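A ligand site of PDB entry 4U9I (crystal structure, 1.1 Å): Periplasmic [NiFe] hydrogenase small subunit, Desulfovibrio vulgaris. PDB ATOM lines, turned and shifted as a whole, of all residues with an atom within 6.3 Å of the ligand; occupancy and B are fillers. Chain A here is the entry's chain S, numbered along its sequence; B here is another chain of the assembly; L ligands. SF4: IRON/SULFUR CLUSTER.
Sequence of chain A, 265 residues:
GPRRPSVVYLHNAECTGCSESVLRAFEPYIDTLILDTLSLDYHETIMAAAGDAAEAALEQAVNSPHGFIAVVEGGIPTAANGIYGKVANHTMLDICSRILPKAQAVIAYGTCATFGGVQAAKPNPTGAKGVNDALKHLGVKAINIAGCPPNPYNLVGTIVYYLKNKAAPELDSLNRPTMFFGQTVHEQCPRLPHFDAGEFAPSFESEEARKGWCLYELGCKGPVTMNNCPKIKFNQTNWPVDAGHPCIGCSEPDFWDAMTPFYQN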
ATOM      1  N   ALA A  13     -36.399 -11.344 -21.991  1.00  0.00           N
ATOM      2  CA  ALA A  13     -35.191 -10.539 -22.133  1.00  0.00           C
ATOM      3  C   ALA A  13     -34.067 -11.259 -21.428  1.00  0.00           C
ATOM      4  O   ALA A  13     -33.956 -11.227 -20.195  1.00  0.00           O
ATOM      5  CB  ALA A  13     -35.370  -9.124 -21.596  1.00  0.00           C
ATOM      6  N   GLU A  14     -33.257 -11.985 -22.216  1.00  0.00           N
ATOM      7  CA  GLU A  14     -32.336 -12.981 -21.697  1.00  0.00           C
ATOM      8  C   GLU A  14     -31.116 -13.080 -22.592  1.00  0.00           C
ATOM      9  O   GLU A  14     -31.144 -12.643 -23.744  1.00  0.00           O
ATOM     10  CB  GLU A  14     -33.016 -14.361 -21.513  1.00  0.00           C
ATOM     11  CG  GLU A  14     -33.881 -14.858 -22.623  1.00  0.00           C
ATOM     12  CD  GLU A  14     -33.154 -15.475 -23.772  1.00  0.00           C
ATOM     13  OE1 GLU A  14     -32.194 -16.243 -23.539  1.00  0.00           O
ATOM     14  OE2 GLU A  14     -33.608 -15.277 -24.989  1.00  0.00           O
ATOM     15  N   CYS A  15     -30.066 -13.692 -22.051  1.00  0.00           N
ATOM     16  CA  CYS A  15     -28.820 -13.891 -22.778  1.00  0.00           C
ATOM     17  C   CYS A  15     -28.634 -15.350 -23.203  1.00  0.00           C
ATOM     18  O   CYS A  15     -27.647 -15.675 -23.870  1.00  0.00           O
ATOM     19  CB  CYS A  15     -27.614 -13.428 -21.969  1.00  0.00           C
ATOM     20  SG  CYS A  15     -27.053 -14.614 -20.695  1.00  0.00           S
ATOM     21  N   THR A  16     -29.544 -16.229 -22.765  1.00  0.00           N
ATOM     22  CA  THR A  16     -29.517 -17.667 -23.066  1.00  0.00           C
ATOM     23  C   THR A  16     -28.496 -18.412 -22.230  1.00  0.00           C
ATOM     24  O   THR A  16     -28.354 -19.626 -22.327  1.00  0.00           O
ATOM     25  CB  THR A  16     -29.445 -17.949 -24.579  1.00  0.00           C
ATOM     26  OG1 THR A  16     -30.365 -17.062 -25.226  1.00  0.00           O
ATOM     27  CG2 THR A  16     -29.772 -19.341 -24.962  1.00  0.00           C
ATOM     28  N   GLY A  17     -27.823 -17.715 -21.316  1.00  0.00           N
ATOM     29  CA  GLY A  17     -26.956 -18.399 -20.364  1.00  0.00           C
ATOM     30  C   GLY A  17     -27.702 -19.312 -19.416  1.00  0.00           C
ATOM     31  O   GLY A  17     -27.156 -20.360 -18.999  1.00  0.00           O
ATOM     32  N   CYS A  18     -28.938 -18.968 -19.052  1.00  0.00           N
ATOM     33  CA  CYS A  18     -29.731 -19.845 -18.218  1.00  0.00           C
ATOM     34  C   CYS A  18     -30.098 -21.121 -18.993  1.00  0.00           C
ATOM     35  O   CYS A  18     -29.957 -22.228 -18.481  1.00  0.00           O
ATOM     36  CB  CYS A  18     -30.950 -19.106 -17.679  1.00  0.00           C
ATOM     37  SG  CYS A  18     -30.553 -17.919 -16.366  1.00  0.00           S
ATOM     38  N   SER A  19     -30.486 -21.003 -20.257  1.00  0.00           N
ATOM     39  CA  SER A  19     -30.742 -22.194 -21.083  1.00  0.00           C
ATOM     40  C   SER A  19     -29.495 -23.064 -21.170  1.00  0.00           C
ATOM     41  O   SER A  19     -29.571 -24.301 -21.029  1.00  0.00           O
ATOM     42  CB  SER A  19     -31.136 -21.826 -22.520  1.00  0.00           C
ATOM     43  OG  SER A  19     -32.468 -21.387 -22.638  1.00  0.00           O
ATOM     44  N   GLU A  73     -37.159 -17.865 -18.511  1.00  0.00           N
ATOM     45  CA  GLU A  73     -35.834 -17.267 -18.552  1.00  0.00           C
ATOM     46  C   GLU A  73     -35.973 -15.849 -19.083  1.00  0.00           C
ATOM     47  O   GLU A  73     -36.648 -15.612 -20.084  1.00  0.00           O
ATOM     48  CB  GLU A  73     -34.926 -18.096 -19.479  1.00  0.00           C
ATOM     49  CG  GLU A  73     -33.522 -17.567 -19.722  1.00  0.00           C
ATOM     50  CD  GLU A  73     -32.656 -18.498 -20.543  1.00  0.00           C
ATOM     51  OE1 GLU A  73     -33.155 -19.569 -20.927  1.00  0.00           O
ATOM     52  OE2 GLU A  73     -31.437 -18.184 -20.734  1.00  0.00           O
ATOM     53  N   GLY A  74     -35.338 -14.915 -18.388  1.00  0.00           N
ATOM     54  CA  GLY A  74     -35.348 -13.541 -18.800  1.00  0.00           C
ATOM     55  C   GLY A  74     -36.338 -12.645 -18.102  1.00  0.00           C
ATOM     56  O   GLY A  74     -37.391 -13.076 -17.647  1.00  0.00           O
ATOM     57  N   GLY A  75     -35.980 -11.353 -18.044  1.00  0.00           N
ATOM     58  CA  GLY A  75     -36.878 -10.342 -17.522  1.00  0.00           C
ATOM     59  C   GLY A  75     -37.964  -9.987 -18.519  1.00  0.00           C
ATOM     60  O   GLY A  75     -37.808 -10.198 -19.719  1.00  0.00           O
ATOM     61  N   TYR A 109     -36.391 -18.835 -13.675  1.00  0.00           N
ATOM     62  CA  TYR A 109     -35.059 -19.411 -13.674  1.00  0.00           C
ATOM     63  C   TYR A 109     -34.054 -18.350 -14.131  1.00  0.00           C
ATOM     64  O   TYR A 109     -34.109 -17.904 -15.279  1.00  0.00           O
ATOM     65  CB  TYR A 109     -35.017 -20.656 -14.553  1.00  0.00           C
ATOM     66  CG  TYR A 109     -33.689 -21.387 -14.474  1.00  0.00           C
ATOM     67  CD1 TYR A 109     -33.248 -21.915 -13.265  1.00  0.00           C
ATOM     68  CD2 TYR A 109     -32.890 -21.572 -15.585  1.00  0.00           C
ATOM     69  CE1 TYR A 109     -31.999 -22.553 -13.165  1.00  0.00           C
ATOM     70  CE2 TYR A 109     -31.683 -22.206 -15.526  1.00  0.00           C
ATOM     71  CZ  TYR A 109     -31.237 -22.699 -14.306  1.00  0.00           C
ATOM     72  OH  TYR A 109     -30.035 -23.352 -14.126  1.00  0.00           O
ATOM     73  N   GLY A 110     -33.173 -17.976 -13.227  1.00  0.00           N
ATOM     74  CA  GLY A 110     -32.162 -16.949 -13.423  1.00  0.00           C
ATOM     75  C   GLY A 110     -32.586 -15.620 -12.823  1.00  0.00           C
ATOM     76  O   GLY A 110     -33.753 -15.266 -12.782  1.00  0.00           O
ATOM     77  N   THR A 111     -31.579 -14.876 -12.363  1.00  0.00           N
ATOM     78  CA  THR A 111     -31.784 -13.559 -11.782  1.00  0.00           C
ATOM     79  C   THR A 111     -32.606 -12.591 -12.637  1.00  0.00           C
ATOM     80  O   THR A 111     -33.350 -11.789 -12.131  1.00  0.00           O
ATOM     81  CB  THR A 111     -30.430 -12.981 -11.349  1.00  0.00           C
ATOM     82  OG1 THR A 111     -29.992 -13.844 -10.296  1.00  0.00           O
ATOM     83  CG2 THR A 111     -30.520 -11.559 -10.843  1.00  0.00           C
ATOM     84  N   CYS A 112     -32.487 -12.690 -13.958  1.00  0.00           N
ATOM     85  CA  CYS A 112     -33.350 -11.873 -14.806  1.00  0.00           C
ATOM     86  C   CYS A 112     -34.842 -12.176 -14.606  1.00  0.00           C
ATOM     87  O   CYS A 112     -35.660 -11.269 -14.359  1.00  0.00           O
ATOM     88  CB  CYS A 112     -32.995 -12.030 -16.297  1.00  0.00           C
ATOM     89  SG  CYS A 112     -31.353 -11.412 -16.738  1.00  0.00           S
ATOM     90  N   ALA A 113     -35.212 -13.445 -14.751  1.00  0.00           N
ATOM     91  CA  ALA A 113     -36.602 -13.851 -14.543  1.00  0.00           C
ATOM     92  C   ALA A 113     -37.060 -13.625 -13.102  1.00  0.00           C
ATOM     93  O   ALA A 113     -38.210 -13.313 -12.865  1.00  0.00           O
ATOM     94  CB  ALA A 113     -36.796 -15.279 -14.972  1.00  0.00           C
ATOM     95  N   GLY A 117     -32.813  -8.558 -13.370  1.00  0.00           N
ATOM     96  CA  GLY A 117     -31.539  -8.865 -14.006  1.00  0.00           C
ATOM     97  C   GLY A 117     -30.843  -7.714 -14.722  1.00  0.00           C
ATOM     98  O   GLY A 117     -31.057  -6.539 -14.436  1.00  0.00           O
ATOM     99  N   VAL A 118     -29.988  -8.091 -15.653  1.00  0.00           N
ATOM    100  CA  VAL A 118     -29.007  -7.155 -16.159  1.00  0.00           C
ATOM    101  C   VAL A 118     -29.689  -5.975 -16.877  1.00  0.00           C
ATOM    102  O   VAL A 118     -29.272  -4.839 -16.712  1.00  0.00           O
ATOM    103  CB  VAL A 118     -27.962  -7.857 -17.049  1.00  0.00           C
ATOM    104  CG1 VAL A 118     -28.550  -8.428 -18.334  1.00  0.00           C
ATOM    105  CG2 VAL A 118     -26.779  -6.916 -17.327  1.00  0.00           C
ATOM    106  N   GLN A 119     -30.749  -6.262 -17.645  1.00  0.00           N
ATOM    107  CA  GLN A 119     -31.441  -5.201 -18.369  1.00  0.00           C
ATOM    108  C   GLN A 119     -32.250  -4.299 -17.443  1.00  0.00           C
ATOM    109  O   GLN A 119     -32.638  -3.195 -17.825  1.00  0.00           O
ATOM    110  CB  GLN A 119     -32.324  -5.750 -19.494  1.00  0.00           C
ATOM    111  CG  GLN A 119     -33.349  -6.780 -19.090  1.00  0.00           C
ATOM    112  CD  GLN A 119     -32.775  -8.169 -19.052  1.00  0.00           C
ATOM    113  OE1 GLN A 119     -32.036  -8.567 -19.956  1.00  0.00           O
ATOM    114  NE2 GLN A 119     -33.083  -8.932 -17.994  1.00  0.00           N
ATOM    115  N   GLY A 147     -29.523 -16.611  -9.615  1.00  0.00           N
ATOM    116  CA  GLY A 147     -28.168 -16.804 -10.081  1.00  0.00           C
ATOM    117  C   GLY A 147     -28.074 -16.380 -11.544  1.00  0.00           C
ATOM    118  O   GLY A 147     -29.086 -16.348 -12.287  1.00  0.00           O
ATOM    119  N   CYS A 148     -26.848 -16.087 -11.982  1.00  0.00           N
ATOM    120  CA  CYS A 148     -26.602 -15.480 -13.307  1.00  0.00           C
ATOM    121  C   CYS A 148     -25.478 -16.195 -14.067  1.00  0.00           C
ATOM    122  O   CYS A 148     -24.400 -15.656 -14.310  1.00  0.00           O
ATOM    123  CB  CYS A 148     -26.347 -13.985 -13.173  1.00  0.00           C
ATOM    124  SG  CYS A 148     -26.482 -12.988 -14.673  1.00  0.00           S
ATOM    125  N   PRO A 149     -25.733 -17.440 -14.510  1.00  0.00           N
ATOM    126  CA  PRO A 149     -26.957 -18.228 -14.299  1.00  0.00           C
ATOM    127  C   PRO A 149     -26.950 -19.017 -12.994  1.00  0.00           C
ATOM    128  O   PRO A 149     -25.911 -19.153 -12.357  1.00  0.00           O
ATOM    129  CB  PRO A 149     -26.956 -19.180 -15.506  1.00  0.00           C
ATOM    130  CG  PRO A 149     -25.509 -19.454 -15.685  1.00  0.00           C
ATOM    131  CD  PRO A 149     -24.786 -18.151 -15.380  1.00  0.00           C
ATOM    132  N   PRO A 150     -28.109 -19.557 -12.623  1.00  0.00           N
ATOM    133  CA  PRO A 150     -28.147 -20.434 -11.439  1.00  0.00           C
ATOM    134  C   PRO A 150     -27.395 -21.708 -11.662  1.00  0.00           C
ATOM    135  O   PRO A 150     -27.037 -22.112 -12.780  1.00  0.00           O
ATOM    136  CB  PRO A 150     -29.649 -20.757 -11.266  1.00  0.00           C
ATOM    137  CG  PRO A 150     -30.344 -19.706 -12.108  1.00  0.00           C
ATOM    138  CD  PRO A 150     -29.417 -19.464 -13.257  1.00  0.00           C
ATOM    139  N   TRP A 256     -26.651  -5.925  -9.806  1.00  0.00           N
ATOM    140  CA  TRP A 256     -25.936  -5.028 -10.716  1.00  0.00           C
ATOM    141  C   TRP A 256     -25.756  -3.631 -10.140  1.00  0.00           C
ATOM    142  O   TRP A 256     -24.768  -2.961 -10.425  1.00  0.00           O
ATOM    143  CB  TRP A 256     -26.684  -4.944 -12.077  1.00  0.00           C
ATOM    144  CG  TRP A 256     -26.807  -6.306 -12.707  1.00  0.00           C
ATOM    145  CD1 TRP A 256     -27.894  -7.103 -12.763  1.00  0.00           C
ATOM    146  CD2 TRP A 256     -25.743  -7.020 -13.350  1.00  0.00           C
ATOM    147  NE1 TRP A 256     -27.581  -8.301 -13.404  1.00  0.00           N
ATOM    148  CE2 TRP A 256     -26.262  -8.248 -13.783  1.00  0.00           C
ATOM    149  CE3 TRP A 256     -24.394  -6.735 -13.573  1.00  0.00           C
ATOM    150  CZ2 TRP A 256     -25.468  -9.215 -14.424  1.00  0.00           C
ATOM    151  CZ3 TRP A 256     -23.609  -7.660 -14.212  1.00  0.00           C
ATOM    152  CH2 TRP A 256     -24.151  -8.916 -14.632  1.00  0.00           C
ATOM    153  N   ARG B  40     -32.157  -4.733 -25.079  1.00  0.00           N
ATOM    154  CA  ARG B  40     -31.865  -4.616 -23.645  1.00  0.00           C
ATOM    155  C   ARG B  40     -31.190  -3.301 -23.273  1.00  0.00           C
ATOM    156  O   ARG B  40     -31.504  -2.734 -22.231  1.00  0.00           O
ATOM    157  CB  ARG B  40     -31.042  -5.823 -23.168  1.00  0.00           C
ATOM    158  CG  ARG B  40     -31.855  -7.111 -23.153  1.00  0.00           C
ATOM    159  CD  ARG B  40     -31.035  -8.373 -22.798  1.00  0.00           C
ATOM    160  NE  ARG B  40     -30.070  -8.599 -23.842  1.00  0.00           N
ATOM    161  CZ  ARG B  40     -28.899  -9.189 -23.652  1.00  0.00           C
ATOM    162  NH1 ARG B  40     -28.569  -9.810 -22.543  1.00  0.00           N
ATOM    163  NH2 ARG B  40     -28.020  -9.168 -24.660  1.00  0.00           N
ATOM    164  N   ARG B  60     -22.881 -10.728 -19.946  1.00  0.00           N
ATOM    165  CA  ARG B  60     -24.295 -11.056 -20.017  1.00  0.00           C
ATOM    166  C   ARG B  60     -24.953 -10.565 -21.306  1.00  0.00           C
ATOM    167  O   ARG B  60     -26.140 -10.689 -21.476  1.00  0.00           O
ATOM    168  CB  ARG B  60     -25.048 -10.573 -18.782  1.00  0.00           C
ATOM    169  CG  ARG B  60     -24.918 -11.462 -17.553  1.00  0.00           C
ATOM    170  CD  ARG B  60     -23.499 -11.587 -17.078  1.00  0.00           C
ATOM    171  NE  ARG B  60     -23.485 -12.373 -15.845  1.00  0.00           N
ATOM    172  CZ  ARG B  60     -22.397 -12.681 -15.137  1.00  0.00           C
ATOM    173  NH1 ARG B  60     -21.243 -12.087 -15.397  1.00  0.00           N
ATOM    174  NH2 ARG B  60     -22.462 -13.584 -14.170  1.00  0.00           N
ATOM    175  N   GLY B  63     -24.913 -15.749 -23.272  1.00  0.00           N
ATOM    176  CA  GLY B  63     -24.500 -16.948 -22.553  1.00  0.00           C
ATOM    177  C   GLY B  63     -24.230 -18.122 -23.479  1.00  0.00           C
ATOM    178  O   GLY B  63     -23.788 -19.164 -22.953  1.00  0.00           O
ATOM    179  N   PRO B 215     -22.039 -21.690 -17.606  1.00  0.00           N
ATOM    180  CA  PRO B 215     -21.783 -20.397 -18.258  1.00  0.00           C
ATOM    181  C   PRO B 215     -21.293 -19.306 -17.333  1.00  0.00           C
ATOM    182  O   PRO B 215     -21.478 -19.329 -16.100  1.00  0.00           O
ATOM    183  CB  PRO B 215     -23.145 -20.007 -18.851  1.00  0.00           C
ATOM    184  CG  PRO B 215     -23.916 -21.311 -18.935  1.00  0.00           C
ATOM    185  CD  PRO B 215     -23.450 -22.088 -17.710  1.00  0.00           C
ATOM    186  N   HIS B 216     -20.701 -18.304 -17.998  1.00  0.00           N
ATOM    187  CA  HIS B 216     -20.298 -17.002 -17.435  1.00  0.00           C
ATOM    188  C   HIS B 216     -19.083 -17.192 -16.494  1.00  0.00           C
ATOM    189  O   HIS B 216     -19.179 -17.329 -15.278  1.00  0.00           O
ATOM    190  CB  HIS B 216     -21.448 -16.214 -16.831  1.00  0.00           C
ATOM    191  CG  HIS B 216     -22.443 -15.740 -17.835  1.00  0.00           C
ATOM    192  ND1 HIS B 216     -22.118 -15.609 -19.184  1.00  0.00           N
ATOM    193  CD2 HIS B 216     -23.724 -15.312 -17.695  1.00  0.00           C
ATOM    194  CE1 HIS B 216     -23.179 -15.117 -19.804  1.00  0.00           C
ATOM    195  NE2 HIS B 216     -24.163 -14.948 -18.934  1.00  0.00           N
HETATM  196 FE1  SF4 L   1     -28.315 -14.375 -18.813  1.00  0.00          FE
HETATM  197 FE2  SF4 L   1     -30.167 -13.319 -17.209  1.00  0.00          FE
HETATM  198 FE3  SF4 L   1     -27.844 -14.026 -16.191  1.00  0.00          FE
HETATM  199 FE4  SF4 L   1     -29.570 -15.990 -17.025  1.00  0.00          FE
HETATM  200  S1  SF4 L   1     -29.912 -14.565 -15.287  1.00  0.00           S
HETATM  201  S2  SF4 L   1     -27.283 -15.903 -17.372  1.00  0.00           S
HETATM  202  S3  SF4 L   1     -30.597 -14.883 -18.816  1.00  0.00           S
HETATM  203  S4  SF4 L   1     -28.168 -12.373 -17.818  1.00  0.00           S
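A sulfur (S1) of the ligand lies close to the backbone carbonyl oxygen (O) of Gly 147 (3.6 Å).
S2 of the ligand sits close to N of Pro 149.
CB of Glu 14 touches S3 of the ligand (3.7 Å).
Gly 17 touches the ligand.
OE2 of Glu 73 touches S3 of the ligand, at 3.9 Å.
Gly 110 touches the ligand.
Val 118 touches the ligand (CG1 to S4, 3.997 Å).
Arg 60 of chain B touches the ligand (CG to S4, 3.4 Å).
A ring nitrogen (NE2) of His 216 of chain B sits close to the side-chain sulfur (SG) of Cys 15, at 3.4 Å.
O of Cys 15 lies within hydrogen-bond range of N of Gly 63 of chain B (2.8 Å).
The guanidinium group (NH2) of Arg 60 of chain B lies within hydrogen-bond range of the backbone carbonyl oxygen (O) of Cys 148, 2.8 Å away.
SG of Cys 112 lies close to N of Val 118 (3.8 Å).
The side-chain sulfur (SG) of Cys 15 sits close to the backbone NH (N) of Gly 17, 3.3 Å away.
The side-chain hydroxyl of Thr 111 is in hydrogen-bond range of the backbone NH of Gly 147 (2.9 Å).
O of Arg 60 of chain B is in hydrogen-bond range of NH1 of Arg 40 of chain B.
The side-chain sulfur (SG) of Cys 18 sits close to the backbone carbonyl oxygen (O) of Tyr 109 (3.7 Å).
The side-chain sulfur (SG) of Cys 148 binds an iron atom (FE3) of the ligand, 2.3 Å away.
SG of Cys 18 is bound to FE4 of the ligand (2.3 Å).
S1 of the ligand lies close to N of Thr 111, at 3.4 Å.
FE1 of the ligand is bound by SG of Cys 15 (2.3 Å).
The backbone NH (N) of Cys 112 lies close to a sulfur (S1) of the ligand, at 3.5 Å.
The side-chain sulfur (SG) of Cys 112 is bound to an iron atom (FE2) of the ligand, 2.3 Å away.
NE2 of His 216 of chain B lies close to S2 of the ligand, at 3.6 Å.
S3 of the ligand sits close to N of Cys 15 (3.5 Å).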
